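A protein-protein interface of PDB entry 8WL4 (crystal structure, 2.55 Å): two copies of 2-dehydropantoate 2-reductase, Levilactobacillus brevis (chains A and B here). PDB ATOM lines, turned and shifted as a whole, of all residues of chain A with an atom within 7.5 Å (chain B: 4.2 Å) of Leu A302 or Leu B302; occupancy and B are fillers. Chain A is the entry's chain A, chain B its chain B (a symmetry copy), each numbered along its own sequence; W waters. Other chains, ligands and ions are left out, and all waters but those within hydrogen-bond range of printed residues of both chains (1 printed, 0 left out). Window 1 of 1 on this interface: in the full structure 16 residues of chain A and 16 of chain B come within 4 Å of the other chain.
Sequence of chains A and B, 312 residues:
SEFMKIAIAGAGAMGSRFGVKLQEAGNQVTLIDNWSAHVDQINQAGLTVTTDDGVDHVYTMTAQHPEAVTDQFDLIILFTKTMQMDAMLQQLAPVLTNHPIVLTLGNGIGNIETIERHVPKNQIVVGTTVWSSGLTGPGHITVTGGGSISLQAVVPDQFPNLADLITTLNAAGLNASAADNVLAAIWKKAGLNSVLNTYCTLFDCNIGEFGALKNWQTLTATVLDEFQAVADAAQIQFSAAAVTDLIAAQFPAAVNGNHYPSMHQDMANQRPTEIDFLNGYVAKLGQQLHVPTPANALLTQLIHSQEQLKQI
Tyr A199 touches Leu B302, and with the chains exchanged Leu A302 touches Tyr B199.
Phe A203 touches Leu B302, and with the chains exchanged Leu A302 touches Phe B203.
Leu A298 touches Leu B299, and with the chains exchanged Leu A299 touches Leu B298.
Leu A302 touches its own counterpart, Leu B302.
Positions printed for both chains: 199, 202, 203, 298, 299, 300, 301, 302, 303, 304, 305 and 306.
The side-chain amide oxygen (OE1) of Gln B301 lies within hydrogen-bond range of the side-chain amide nitrogen (ND2) of Asn A215 (2.7 Å).
The side-chain amide oxygen of Asn A215 sits at hydrogen-bond distance from the side-chain hydroxyl of Ser B305, at 2.7 Å.
Water W1 bridges O of Phe A203 (3.0 Å) and NE2 of Gln B306 (3.3 Å).
Leu A302 touches just these residues of chain B: Tyr B199, Phe B203 and Leu B302.
Leu B302 touches just these residues of chain A: Tyr A199, Phe A203 and Leu A302.
Printed residues of chain A within 4 Å of Leu B299: Leu A298 (3.97 Å).
Of the printed residues of chain A, Leu B298 touches Ala A295 (3.9 Å) and Leu A299 (3.9 Å).
Printed residues of chain B within 4 Å of Ala A295: Leu B298.
Gln A301 touches none of the printed residues of chain B.
The nearest printed residue of chain A that does not touch Ser B305 is Tyr A199 (6.9 Å).
Leu B302 touches Tyr A199.
CB of Ser B305 touches CZ of Phe A203, at 3.5 Å.
Gln B301 touches Leu A219.
CD1 of Leu A219 touches OG of Ser B305, at 3.4 Å.
Leu B298 touches Ala A295 (CD2 to O, 3.9 Å).
Leu A298 touches Leu B299.
Leu A302 touches Phe B203 (O to CE1, 3.6 Å).
Leu A302 touches Leu B302.
Ser A305 touches Phe B203.
Phe B203 touches Leu A309.
O of Gln B301 sits at hydrogen-bond distance from OG of Ser B305 (3.2 Å).
The side-chain hydroxyl of Tyr A199 sits at hydrogen-bond distance from the backbone carbonyl oxygen of Leu A219.
The backbone carbonyl oxygen (O) of Gln A301 is in hydrogen-bond range of the side-chain hydroxyl (OG) of Ser A305, at 3.2 Å.
Of the 12 printed residues of chain B, 7 touch a printed residue of chain A.
Of the 24 printed residues of chain A, 11 touch a printed residue of chain B.
Hydrophobic or aromatic side chains of chain A within 4 Å of the printed part of chain B: Tyr A199, Phe A203, Leu A213, Leu A219, Ala A295, Leu A298, Leu A299, Leu A302 and Leu A309.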
ATOM      1  N   THR A 198      11.433  -1.480  10.730  1.00  0.00           N
ATOM      2  CA  THR A 198      12.105  -0.207  11.019  1.00  0.00           C
ATOM      3  C   THR A 198      13.303   0.064  10.099  1.00  0.00           C
ATOM      4  O   THR A 198      13.389   1.128   9.482  1.00  0.00           O
ATOM      5  CB  THR A 198      12.584  -0.163  12.493  1.00  0.00           C
ATOM      6  OG1 THR A 198      11.454  -0.285  13.372  1.00  0.00           O
ATOM      7  CG2 THR A 198      13.283   1.126  12.784  1.00  0.00           C
ATOM      8  N   TYR A 199      14.233  -0.877  10.024  1.00  0.00           N
ATOM      9  CA  TYR A 199      15.436  -0.693   9.217  1.00  0.00           C
ATOM     10  C   TYR A 199      15.143  -0.651   7.722  1.00  0.00           C
ATOM     11  O   TYR A 199      15.742   0.128   6.988  1.00  0.00           O
ATOM     12  CB  TYR A 199      16.468  -1.781   9.525  1.00  0.00           C
ATOM     13  CG  TYR A 199      17.197  -1.645  10.862  1.00  0.00           C
ATOM     14  CD1 TYR A 199      17.948  -0.510  11.166  1.00  0.00           C
ATOM     15  CD2 TYR A 199      17.194  -2.685  11.782  1.00  0.00           C
ATOM     16  CE1 TYR A 199      18.657  -0.406  12.355  1.00  0.00           C
ATOM     17  CE2 TYR A 199      17.892  -2.595  12.987  1.00  0.00           C
ATOM     18  CZ  TYR A 199      18.623  -1.453  13.265  1.00  0.00           C
ATOM     19  OH  TYR A 199      19.312  -1.360  14.447  1.00  0.00           O
ATOM     20  N   LEU A 202      13.846   2.700   7.057  1.00  0.00           N
ATOM     21  CA  LEU A 202      14.917   3.669   7.131  1.00  0.00           C
ATOM     22  C   LEU A 202      15.831   3.594   5.921  1.00  0.00           C
ATOM     23  O   LEU A 202      16.320   4.616   5.466  1.00  0.00           O
ATOM     24  CB  LEU A 202      15.734   3.482   8.400  1.00  0.00           C
ATOM     25  CG  LEU A 202      15.162   4.146   9.642  1.00  0.00           C
ATOM     26  CD1 LEU A 202      15.786   3.527  10.888  1.00  0.00           C
ATOM     27  CD2 LEU A 202      15.425   5.640   9.654  1.00  0.00           C
ATOM     28  N   PHE A 203      16.079   2.396   5.410  1.00  0.00           N
ATOM     29  CA  PHE A 203      16.971   2.236   4.251  1.00  0.00           C
ATOM     30  C   PHE A 203      16.276   2.243   2.872  1.00  0.00           C
ATOM     31  O   PHE A 203      16.947   2.182   1.860  1.00  0.00           O
ATOM     32  CB  PHE A 203      17.773   0.945   4.403  1.00  0.00           C
ATOM     33  CG  PHE A 203      18.606   0.868   5.662  1.00  0.00           C
ATOM     34  CD1 PHE A 203      19.299   1.971   6.144  1.00  0.00           C
ATOM     35  CD2 PHE A 203      18.755  -0.340   6.327  1.00  0.00           C
ATOM     36  CE1 PHE A 203      20.094   1.876   7.278  1.00  0.00           C
ATOM     37  CE2 PHE A 203      19.541  -0.447   7.469  1.00  0.00           C
ATOM     38  CZ  PHE A 203      20.208   0.659   7.951  1.00  0.00           C
ATOM     39  N   LEU A 213      23.320  -7.036   4.036  1.00  0.00           N
ATOM     40  CA  LEU A 213      24.167  -5.960   4.592  1.00  0.00           C
ATOM     41  C   LEU A 213      25.325  -6.519   5.417  1.00  0.00           C
ATOM     42  O   LEU A 213      25.132  -7.409   6.237  1.00  0.00           O
ATOM     43  CB  LEU A 213      23.340  -4.985   5.470  1.00  0.00           C
ATOM     44  CG  LEU A 213      22.320  -4.022   4.832  1.00  0.00           C
ATOM     45  CD1 LEU A 213      21.557  -3.212   5.865  1.00  0.00           C
ATOM     46  CD2 LEU A 213      23.005  -3.071   3.882  1.00  0.00           C
ATOM     47  N   ASN A 215      26.687  -5.420   7.901  1.00  0.00           N
ATOM     48  CA  ASN A 215      26.463  -5.200   9.338  1.00  0.00           C
ATOM     49  C   ASN A 215      25.041  -5.524   9.868  1.00  0.00           C
ATOM     50  O   ASN A 215      24.646  -5.019  10.917  1.00  0.00           O
ATOM     51  CB  ASN A 215      26.862  -3.760   9.703  1.00  0.00           C
ATOM     52  CG  ASN A 215      25.988  -2.714   9.042  1.00  0.00           C
ATOM     53  OD1 ASN A 215      25.339  -2.973   8.030  1.00  0.00           O
ATOM     54  ND2 ASN A 215      25.979  -1.511   9.606  1.00  0.00           N
ATOM     55  N   LEU A 219      23.278  -4.418  13.615  1.00  0.00           N
ATOM     56  CA  LEU A 219      22.052  -3.627  13.585  1.00  0.00           C
ATOM     57  C   LEU A 219      20.940  -4.376  14.316  1.00  0.00           C
ATOM     58  O   LEU A 219      20.192  -3.809  15.114  1.00  0.00           O
ATOM     59  CB  LEU A 219      21.634  -3.373  12.136  1.00  0.00           C
ATOM     60  CG  LEU A 219      22.471  -2.410  11.272  1.00  0.00           C
ATOM     61  CD1 LEU A 219      21.782  -2.146   9.948  1.00  0.00           C
ATOM     62  CD2 LEU A 219      22.721  -1.091  11.978  1.00  0.00           C
ATOM     63  N   MET A 267       5.009   4.102   4.890  1.00  0.00           N
ATOM     64  CA  MET A 267       5.821   5.294   4.600  1.00  0.00           C
ATOM     65  C   MET A 267       5.670   5.691   3.149  1.00  0.00           C
ATOM     66  O   MET A 267       5.495   6.863   2.853  1.00  0.00           O
ATOM     67  CB  MET A 267       7.310   5.051   4.903  1.00  0.00           C
ATOM     68  CG  MET A 267       8.204   6.290   4.836  1.00  0.00           C
ATOM     69  SD  MET A 267       7.965   7.474   6.180  1.00  0.00           S
ATOM     70  CE  MET A 267       8.463   6.514   7.608  1.00  0.00           C
ATOM     71  N   ILE A 275       5.352   2.783  14.516  1.00  0.00           N
ATOM     72  CA  ILE A 275       6.621   2.879  15.213  1.00  0.00           C
ATOM     73  C   ILE A 275       6.500   3.102  16.721  1.00  0.00           C
ATOM     74  O   ILE A 275       7.269   2.514  17.483  1.00  0.00           O
ATOM     75  CB  ILE A 275       7.509   3.967  14.587  1.00  0.00           C
ATOM     76  CG1 ILE A 275       8.931   3.872  15.141  1.00  0.00           C
ATOM     77  CG2 ILE A 275       6.908   5.360  14.792  1.00  0.00           C
ATOM     78  CD1 ILE A 275       9.616   2.553  14.839  1.00  0.00           C
ATOM     79  N   ALA A 295      19.037   3.233  21.659  1.00  0.00           N
ATOM     80  CA  ALA A 295      18.986   2.851  20.253  1.00  0.00           C
ATOM     81  C   ALA A 295      17.567   2.776  19.743  1.00  0.00           C
ATOM     82  O   ALA A 295      17.259   3.333  18.696  1.00  0.00           O
ATOM     83  CB  ALA A 295      19.703   1.523  20.031  1.00  0.00           C
ATOM     84  N   ASN A 296      16.695   2.100  20.477  1.00  0.00           N
ATOM     85  CA  ASN A 296      15.268   2.097  20.125  1.00  0.00           C
ATOM     86  C   ASN A 296      14.608   3.475  20.289  1.00  0.00           C
ATOM     87  O   ASN A 296      13.727   3.838  19.509  1.00  0.00           O
ATOM     88  CB  ASN A 296      14.496   1.028  20.912  1.00  0.00           C
ATOM     89  CG  ASN A 296      14.677  -0.364  20.330  1.00  0.00           C
ATOM     90  OD1 ASN A 296      14.088  -0.705  19.303  1.00  0.00           O
ATOM     91  ND2 ASN A 296      15.501  -1.175  20.981  1.00  0.00           N
ATOM     92  N   ALA A 297      15.021   4.266  21.272  1.00  0.00           N
ATOM     93  CA  ALA A 297      14.482   5.634  21.341  1.00  0.00           C
ATOM     94  C   ALA A 297      14.867   6.406  20.092  1.00  0.00           C
ATOM     95  O   ALA A 297      14.049   7.163  19.559  1.00  0.00           O
ATOM     96  CB  ALA A 297      14.943   6.370  22.584  1.00  0.00           C
ATOM     97  N   LEU A 298      16.094   6.193  19.615  1.00  0.00           N
ATOM     98  CA  LEU A 298      16.622   6.960  18.486  1.00  0.00           C
ATOM     99  C   LEU A 298      15.968   6.566  17.174  1.00  0.00           C
ATOM    100  O   LEU A 298      15.512   7.423  16.415  1.00  0.00           O
ATOM    101  CB  LEU A 298      18.143   6.819  18.388  1.00  0.00           C
ATOM    102  CG  LEU A 298      18.830   7.501  17.199  1.00  0.00           C
ATOM    103  CD1 LEU A 298      18.483   8.982  17.180  1.00  0.00           C
ATOM    104  CD2 LEU A 298      20.351   7.283  17.210  1.00  0.00           C
ATOM    105  N   LEU A 299      15.907   5.264  16.916  1.00  0.00           N
ATOM    106  CA  LEU A 299      15.275   4.767  15.700  1.00  0.00           C
ATOM    107  C   LEU A 299      13.827   5.255  15.598  1.00  0.00           C
ATOM    108  O   LEU A 299      13.378   5.661  14.533  1.00  0.00           O
ATOM    109  CB  LEU A 299      15.341   3.251  15.661  1.00  0.00           C
ATOM    110  CG  LEU A 299      16.732   2.633  15.554  1.00  0.00           C
ATOM    111  CD1 LEU A 299      16.640   1.128  15.816  1.00  0.00           C
ATOM    112  CD2 LEU A 299      17.372   2.944  14.198  1.00  0.00           C
ATOM    113  N   THR A 300      13.108   5.229  16.718  1.00  0.00           N
ATOM    114  CA  THR A 300      11.781   5.848  16.795  1.00  0.00           C
ATOM    115  C   THR A 300      11.781   7.304  16.333  1.00  0.00           C
ATOM    116  O   THR A 300      10.890   7.715  15.601  1.00  0.00           O
ATOM    117  CB  THR A 300      11.224   5.808  18.234  1.00  0.00           C
ATOM    118  OG1 THR A 300      11.152   4.452  18.689  1.00  0.00           O
ATOM    119  CG2 THR A 300       9.848   6.438  18.296  1.00  0.00           C
ATOM    120  N   GLN A 301      12.752   8.097  16.781  1.00  0.00           N
ATOM    121  CA  GLN A 301      12.834   9.488  16.338  1.00  0.00           C
ATOM    122  C   GLN A 301      13.131   9.576  14.844  1.00  0.00           C
ATOM    123  O   GLN A 301      12.529  10.384  14.140  1.00  0.00           O
ATOM    124  CB  GLN A 301      13.868  10.272  17.131  1.00  0.00           C
ATOM    125  CG  GLN A 301      13.501  10.523  18.589  1.00  0.00           C
ATOM    126  CD  GLN A 301      12.234  11.358  18.749  1.00  0.00           C
ATOM    127  OE1 GLN A 301      12.081  12.407  18.115  1.00  0.00           O
ATOM    128  NE2 GLN A 301      11.313  10.895  19.597  1.00  0.00           N
ATOM    129  N   LEU A 302      14.032   8.732  14.352  1.00  0.00           N
ATOM    130  CA  LEU A 302      14.392   8.778  12.938  1.00  0.00           C
ATOM    131  C   LEU A 302      13.190   8.511  12.036  1.00  0.00           C
ATOM    132  O   LEU A 302      13.038   9.160  11.008  1.00  0.00           O
ATOM    133  CB  LEU A 302      15.510   7.787  12.612  1.00  0.00           C
ATOM    134  CG  LEU A 302      16.851   7.946  13.320  1.00  0.00           C
ATOM    135  CD1 LEU A 302      17.804   6.848  12.866  1.00  0.00           C
ATOM    136  CD2 LEU A 302      17.485   9.302  13.071  1.00  0.00           C
ATOM    137  N   ILE A 303      12.336   7.570  12.419  1.00  0.00           N
ATOM    138  CA  ILE A 303      11.161   7.223  11.614  1.00  0.00           C
ATOM    139  C   ILE A 303      10.124   8.341  11.617  1.00  0.00           C
ATOM    140  O   ILE A 303       9.580   8.675  10.576  1.00  0.00           O
ATOM    141  CB  ILE A 303      10.514   5.913  12.106  1.00  0.00           C
ATOM    142  CG1 ILE A 303      11.441   4.732  11.820  1.00  0.00           C
ATOM    143  CG2 ILE A 303       9.155   5.672  11.450  1.00  0.00           C
ATOM    144  CD1 ILE A 303      11.492   4.294  10.367  1.00  0.00           C
ATOM    145  N   HIS A 304       9.823   8.907  12.774  1.00  0.00           N
ATOM    146  CA  HIS A 304       8.933  10.077  12.815  1.00  0.00           C
ATOM    147  C   HIS A 304       9.430  11.190  11.879  1.00  0.00           C
ATOM    148  O   HIS A 304       8.657  11.762  11.097  1.00  0.00           O
ATOM    149  CB  HIS A 304       8.815  10.620  14.235  1.00  0.00           C
ATOM    150  CG  HIS A 304       8.025   9.743  15.153  1.00  0.00           C
ATOM    151  ND1 HIS A 304       6.964   8.980  14.717  1.00  0.00           N
ATOM    152  CD2 HIS A 304       8.112   9.542  16.490  1.00  0.00           C
ATOM    153  CE1 HIS A 304       6.432   8.342  15.747  1.00  0.00           C
ATOM    154  NE2 HIS A 304       7.119   8.656  16.832  1.00  0.00           N
ATOM    155  N   SER A 305      10.727  11.477  11.944  1.00  0.00           N
ATOM    156  CA  SER A 305      11.316  12.450  11.052  1.00  0.00           C
ATOM    157  C   SER A 305      11.042  12.086   9.603  1.00  0.00           C
ATOM    158  O   SER A 305      10.491  12.896   8.860  1.00  0.00           O
ATOM    159  CB  SER A 305      12.805  12.623  11.344  1.00  0.00           C
ATOM    160  OG  SER A 305      12.982  13.205  12.649  1.00  0.00           O
ATOM    161  N   GLN A 306      11.369  10.861   9.207  1.00  0.00           N
ATOM    162  CA  GLN A 306      11.024  10.364   7.863  1.00  0.00           C
ATOM    163  C   GLN A 306       9.564  10.646   7.496  1.00  0.00           C
ATOM    164  O   GLN A 306       9.295  11.124   6.393  1.00  0.00           O
ATOM    165  CB  GLN A 306      11.289   8.856   7.745  1.00  0.00           C
ATOM    166  CG  GLN A 306      11.919   8.388   6.447  1.00  0.00           C
ATOM    167  CD  GLN A 306      12.425   6.954   6.545  1.00  0.00           C
ATOM    168  OE1 GLN A 306      13.030   6.561   7.551  1.00  0.00           O
ATOM    169  NE2 GLN A 306      12.180   6.157   5.500  1.00  0.00           N
ATOM    170  N   GLU A 307       8.623  10.352   8.398  1.00  0.00           N
ATOM    171  CA  GLU A 307       7.199  10.621   8.115  1.00  0.00           C
ATOM    172  C   GLU A 307       6.967  12.055   7.715  1.00  0.00           C
ATOM    173  O   GLU A 307       6.325  12.344   6.713  1.00  0.00           O
ATOM    174  CB  GLU A 307       6.311  10.337   9.329  1.00  0.00           C
ATOM    175  CG  GLU A 307       5.929   8.881   9.473  1.00  0.00           C
ATOM    176  CD  GLU A 307       4.983   8.644  10.622  1.00  0.00           C
ATOM    177  OE1 GLU A 307       4.112   9.521  10.866  1.00  0.00           O
ATOM    178  OE2 GLU A 307       5.118   7.571  11.266  1.00  0.00           O
ATOM    179  N   GLN A 308       7.497  12.951   8.533  1.00  0.00           N
ATOM    180  CA  GLN A 308       7.286  14.355   8.347  1.00  0.00           C
ATOM    181  C   GLN A 308       7.844  14.826   7.000  1.00  0.00           C
ATOM    182  O   GLN A 308       7.254  15.689   6.357  1.00  0.00           O
ATOM    183  CB  GLN A 308       7.917  15.106   9.510  1.00  0.00           C
ATOM    184  CG  GLN A 308       7.253  16.420   9.851  1.00  0.00           C
ATOM    185  CD  GLN A 308       8.143  17.252  10.737  1.00  0.00           C
ATOM    186  OE1 GLN A 308       8.661  16.751  11.748  1.00  0.00           O
ATOM    187  NE2 GLN A 308       8.350  18.525  10.367  1.00  0.00           N
ATOM    188  N   LEU A 309       8.955  14.243   6.562  1.00  0.00           N
ATOM    189  CA  LEU A 309       9.564  14.598   5.272  1.00  0.00           C
ATOM    190  C   LEU A 309       8.796  14.099   4.061  1.00  0.00           C
ATOM    191  O   LEU A 309       8.805  14.745   3.012  1.00  0.00           O
ATOM    192  CB  LEU A 309      10.989  14.064   5.183  1.00  0.00           C
ATOM    193  CG  LEU A 309      11.963  14.631   6.206  1.00  0.00           C
ATOM    194  CD1 LEU A 309      13.320  13.990   5.993  1.00  0.00           C
ATOM    195  CD2 LEU A 309      12.042  16.147   6.094  1.00  0.00           C
ATOM    196  N   TYR B 199      22.522  13.347   9.595  1.00  0.00           N
ATOM    197  CA  TYR B 199      21.062  13.276   9.514  1.00  0.00           C
ATOM    198  C   TYR B 199      20.534  13.631   8.132  1.00  0.00           C
ATOM    199  O   TYR B 199      19.590  13.008   7.652  1.00  0.00           O
ATOM    200  CB  TYR B 199      20.413  14.177  10.569  1.00  0.00           C
ATOM    201  CG  TYR B 199      20.476  13.660  12.005  1.00  0.00           C
ATOM    202  CD1 TYR B 199      19.916  12.427  12.358  1.00  0.00           C
ATOM    203  CD2 TYR B 199      21.039  14.431  13.016  1.00  0.00           C
ATOM    204  CE1 TYR B 199      19.928  11.978  13.671  1.00  0.00           C
ATOM    205  CE2 TYR B 199      21.069  13.982  14.334  1.00  0.00           C
ATOM    206  CZ  TYR B 199      20.511  12.755  14.658  1.00  0.00           C
ATOM    207  OH  TYR B 199      20.531  12.324  15.957  1.00  0.00           O
ATOM    208  N   LEU B 202      21.061  10.659   6.083  1.00  0.00           N
ATOM    209  CA  LEU B 202      20.126   9.618   6.457  1.00  0.00           C
ATOM    210  C   LEU B 202      18.727   9.912   5.963  1.00  0.00           C
ATOM    211  O   LEU B 202      18.014   8.997   5.583  1.00  0.00           O
ATOM    212  CB  LEU B 202      20.100   9.414   7.961  1.00  0.00           C
ATOM    213  CG  LEU B 202      21.204   8.525   8.509  1.00  0.00           C
ATOM    214  CD1 LEU B 202      21.319   8.757  10.011  1.00  0.00           C
ATOM    215  CD2 LEU B 202      20.946   7.054   8.252  1.00  0.00           C
ATOM    216  N   PHE B 203      18.325  11.177   5.975  1.00  0.00           N
ATOM    217  CA  PHE B 203      16.972  11.544   5.541  1.00  0.00           C
ATOM    218  C   PHE B 203      16.845  11.940   4.053  1.00  0.00           C
ATOM    219  O   PHE B 203      15.745  12.215   3.590  1.00  0.00           O
ATOM    220  CB  PHE B 203      16.461  12.699   6.400  1.00  0.00           C
ATOM    221  CG  PHE B 203      16.416  12.410   7.879  1.00  0.00           C
ATOM    222  CD1 PHE B 203      16.025  11.166   8.374  1.00  0.00           C
ATOM    223  CD2 PHE B 203      16.699  13.416   8.789  1.00  0.00           C
ATOM    224  CE1 PHE B 203      15.954  10.937   9.744  1.00  0.00           C
ATOM    225  CE2 PHE B 203      16.631  13.191  10.161  1.00  0.00           C
ATOM    226  CZ  PHE B 203      16.257  11.955  10.639  1.00  0.00           C
ATOM    227  N   LEU B 298      25.429   3.951  16.616  1.00  0.00           N
ATOM    228  CA  LEU B 298      24.334   3.458  15.773  1.00  0.00           C
ATOM    229  C   LEU B 298      24.241   4.233  14.463  1.00  0.00           C
ATOM    230  O   LEU B 298      24.172   3.639  13.388  1.00  0.00           O
ATOM    231  CB  LEU B 298      23.001   3.496  16.521  1.00  0.00           C
ATOM    232  CG  LEU B 298      21.732   3.144  15.714  1.00  0.00           C
ATOM    233  CD1 LEU B 298      21.857   1.785  15.045  1.00  0.00           C
ATOM    234  CD2 LEU B 298      20.462   3.204  16.563  1.00  0.00           C
ATOM    235  N   LEU B 299      24.250   5.558  14.554  1.00  0.00           N
ATOM    236  CA  LEU B 299      24.216   6.396  13.362  1.00  0.00           C
ATOM    237  C   LEU B 299      25.359   6.046  12.400  1.00  0.00           C
ATOM    238  O   LEU B 299      25.161   5.958  11.192  1.00  0.00           O
ATOM    239  CB  LEU B 299      24.273   7.868  13.756  1.00  0.00           C
ATOM    240  CG  LEU B 299      23.062   8.392  14.536  1.00  0.00           C
ATOM    241  CD1 LEU B 299      23.358   9.767  15.129  1.00  0.00           C
ATOM    242  CD2 LEU B 299      21.820   8.430  13.656  1.00  0.00           C
ATOM    243  N   THR B 300      26.550   5.828  12.946  1.00  0.00           N
ATOM    244  CA  THR B 300      27.674   5.302  12.163  1.00  0.00           C
ATOM    245  C   THR B 300      27.326   4.015  11.420  1.00  0.00           C
ATOM    246  O   THR B 300      27.669   3.870  10.257  1.00  0.00           O
ATOM    247  CB  THR B 300      28.902   5.012  13.057  1.00  0.00           C
ATOM    248  OG1 THR B 300      29.299   6.208  13.736  1.00  0.00           O
ATOM    249  CG2 THR B 300      30.056   4.502  12.230  1.00  0.00           C
ATOM    250  N   GLN B 301      26.672   3.070  12.091  1.00  0.00           N
ATOM    251  CA  GLN B 301      26.250   1.843  11.418  1.00  0.00           C
ATOM    252  C   GLN B 301      25.219   2.124  10.328  1.00  0.00           C
ATOM    253  O   GLN B 301      25.293   1.562   9.241  1.00  0.00           O
ATOM    254  CB  GLN B 301      25.686   0.815  12.396  1.00  0.00           C
ATOM    255  CG  GLN B 301      26.691   0.205  13.361  1.00  0.00           C
ATOM    256  CD  GLN B 301      27.822  -0.537  12.656  1.00  0.00           C
ATOM    257  OE1 GLN B 301      27.604  -1.313  11.720  1.00  0.00           O
ATOM    258  NE2 GLN B 301      29.041  -0.293  13.100  1.00  0.00           N
ATOM    259  N   LEU B 302      24.268   3.009  10.603  1.00  0.00           N
ATOM    260  CA  LEU B 302      23.222   3.290   9.628  1.00  0.00           C
ATOM    261  C   LEU B 302      23.796   3.855   8.332  1.00  0.00           C
ATOM    262  O   LEU B 302      23.344   3.505   7.246  1.00  0.00           O
ATOM    263  CB  LEU B 302      22.180   4.248  10.192  1.00  0.00           C
ATOM    264  CG  LEU B 302      21.394   3.838  11.428  1.00  0.00           C
ATOM    265  CD1 LEU B 302      20.459   4.963  11.839  1.00  0.00           C
ATOM    266  CD2 LEU B 302      20.609   2.562  11.208  1.00  0.00           C
ATOM    267  N   ILE B 303      24.798   4.720   8.441  1.00  0.00           N
ATOM    268  CA  ILE B 303      25.410   5.334   7.260  1.00  0.00           C
ATOM    269  C   ILE B 303      26.201   4.323   6.440  1.00  0.00           C
ATOM    270  O   ILE B 303      26.095   4.291   5.222  1.00  0.00           O
ATOM    271  CB  ILE B 303      26.310   6.518   7.650  1.00  0.00           C
ATOM    272  CG1 ILE B 303      25.456   7.670   8.189  1.00  0.00           C
ATOM    273  CG2 ILE B 303      27.151   7.005   6.472  1.00  0.00           C
ATOM    274  CD1 ILE B 303      24.676   8.438   7.140  1.00  0.00           C
ATOM    275  N   HIS B 304      27.012   3.506   7.090  1.00  0.00           N
ATOM    276  CA  HIS B 304      27.697   2.421   6.374  1.00  0.00           C
ATOM    277  C   HIS B 304      26.699   1.545   5.597  1.00  0.00           C
ATOM    278  O   HIS B 304      26.913   1.234   4.423  1.00  0.00           O
ATOM    279  CB  HIS B 304      28.499   1.552   7.342  1.00  0.00           C
ATOM    280  CG  HIS B 304      29.716   2.223   7.892  1.00  0.00           C
ATOM    281  ND1 HIS B 304      30.436   3.152   7.177  1.00  0.00           N
ATOM    282  CD2 HIS B 304      30.357   2.077   9.074  1.00  0.00           C
ATOM    283  CE1 HIS B 304      31.471   3.553   7.896  1.00  0.00           C
ATOM    284  NE2 HIS B 304      31.440   2.923   9.055  1.00  0.00           N
ATOM    285  N   SER B 305      25.602   1.171   6.248  1.00  0.00           N
ATOM    286  CA  SER B 305      24.562   0.413   5.583  1.00  0.00           C
ATOM    287  C   SER B 305      24.084   1.146   4.343  1.00  0.00           C
ATOM    288  O   SER B 305      24.116   0.575   3.250  1.00  0.00           O
ATOM    289  CB  SER B 305      23.411   0.096   6.539  1.00  0.00           C
ATOM    290  OG  SER B 305      23.861  -0.803   7.564  1.00  0.00           O
ATOM    291  N   GLN B 306      23.698   2.410   4.486  1.00  0.00           N
ATOM    292  CA  GLN B 306      23.351   3.232   3.324  1.00  0.00           C
ATOM    293  C   GLN B 306      24.390   3.149   2.200  1.00  0.00           C
ATOM    294  O   GLN B 306      24.023   2.977   1.041  1.00  0.00           O
ATOM    295  CB  GLN B 306      23.130   4.710   3.720  1.00  0.00           C
ATOM    296  CG  GLN B 306      21.829   4.964   4.466  1.00  0.00           C
ATOM    297  CD  GLN B 306      21.236   6.341   4.202  1.00  0.00           C
ATOM    298  OE1 GLN B 306      21.957   7.348   4.132  1.00  0.00           O
ATOM    299  NE2 GLN B 306      19.911   6.393   4.056  1.00  0.00           N
HETATM  300  O   HOH W   1      19.469   3.869   1.994  1.00  0.00           O
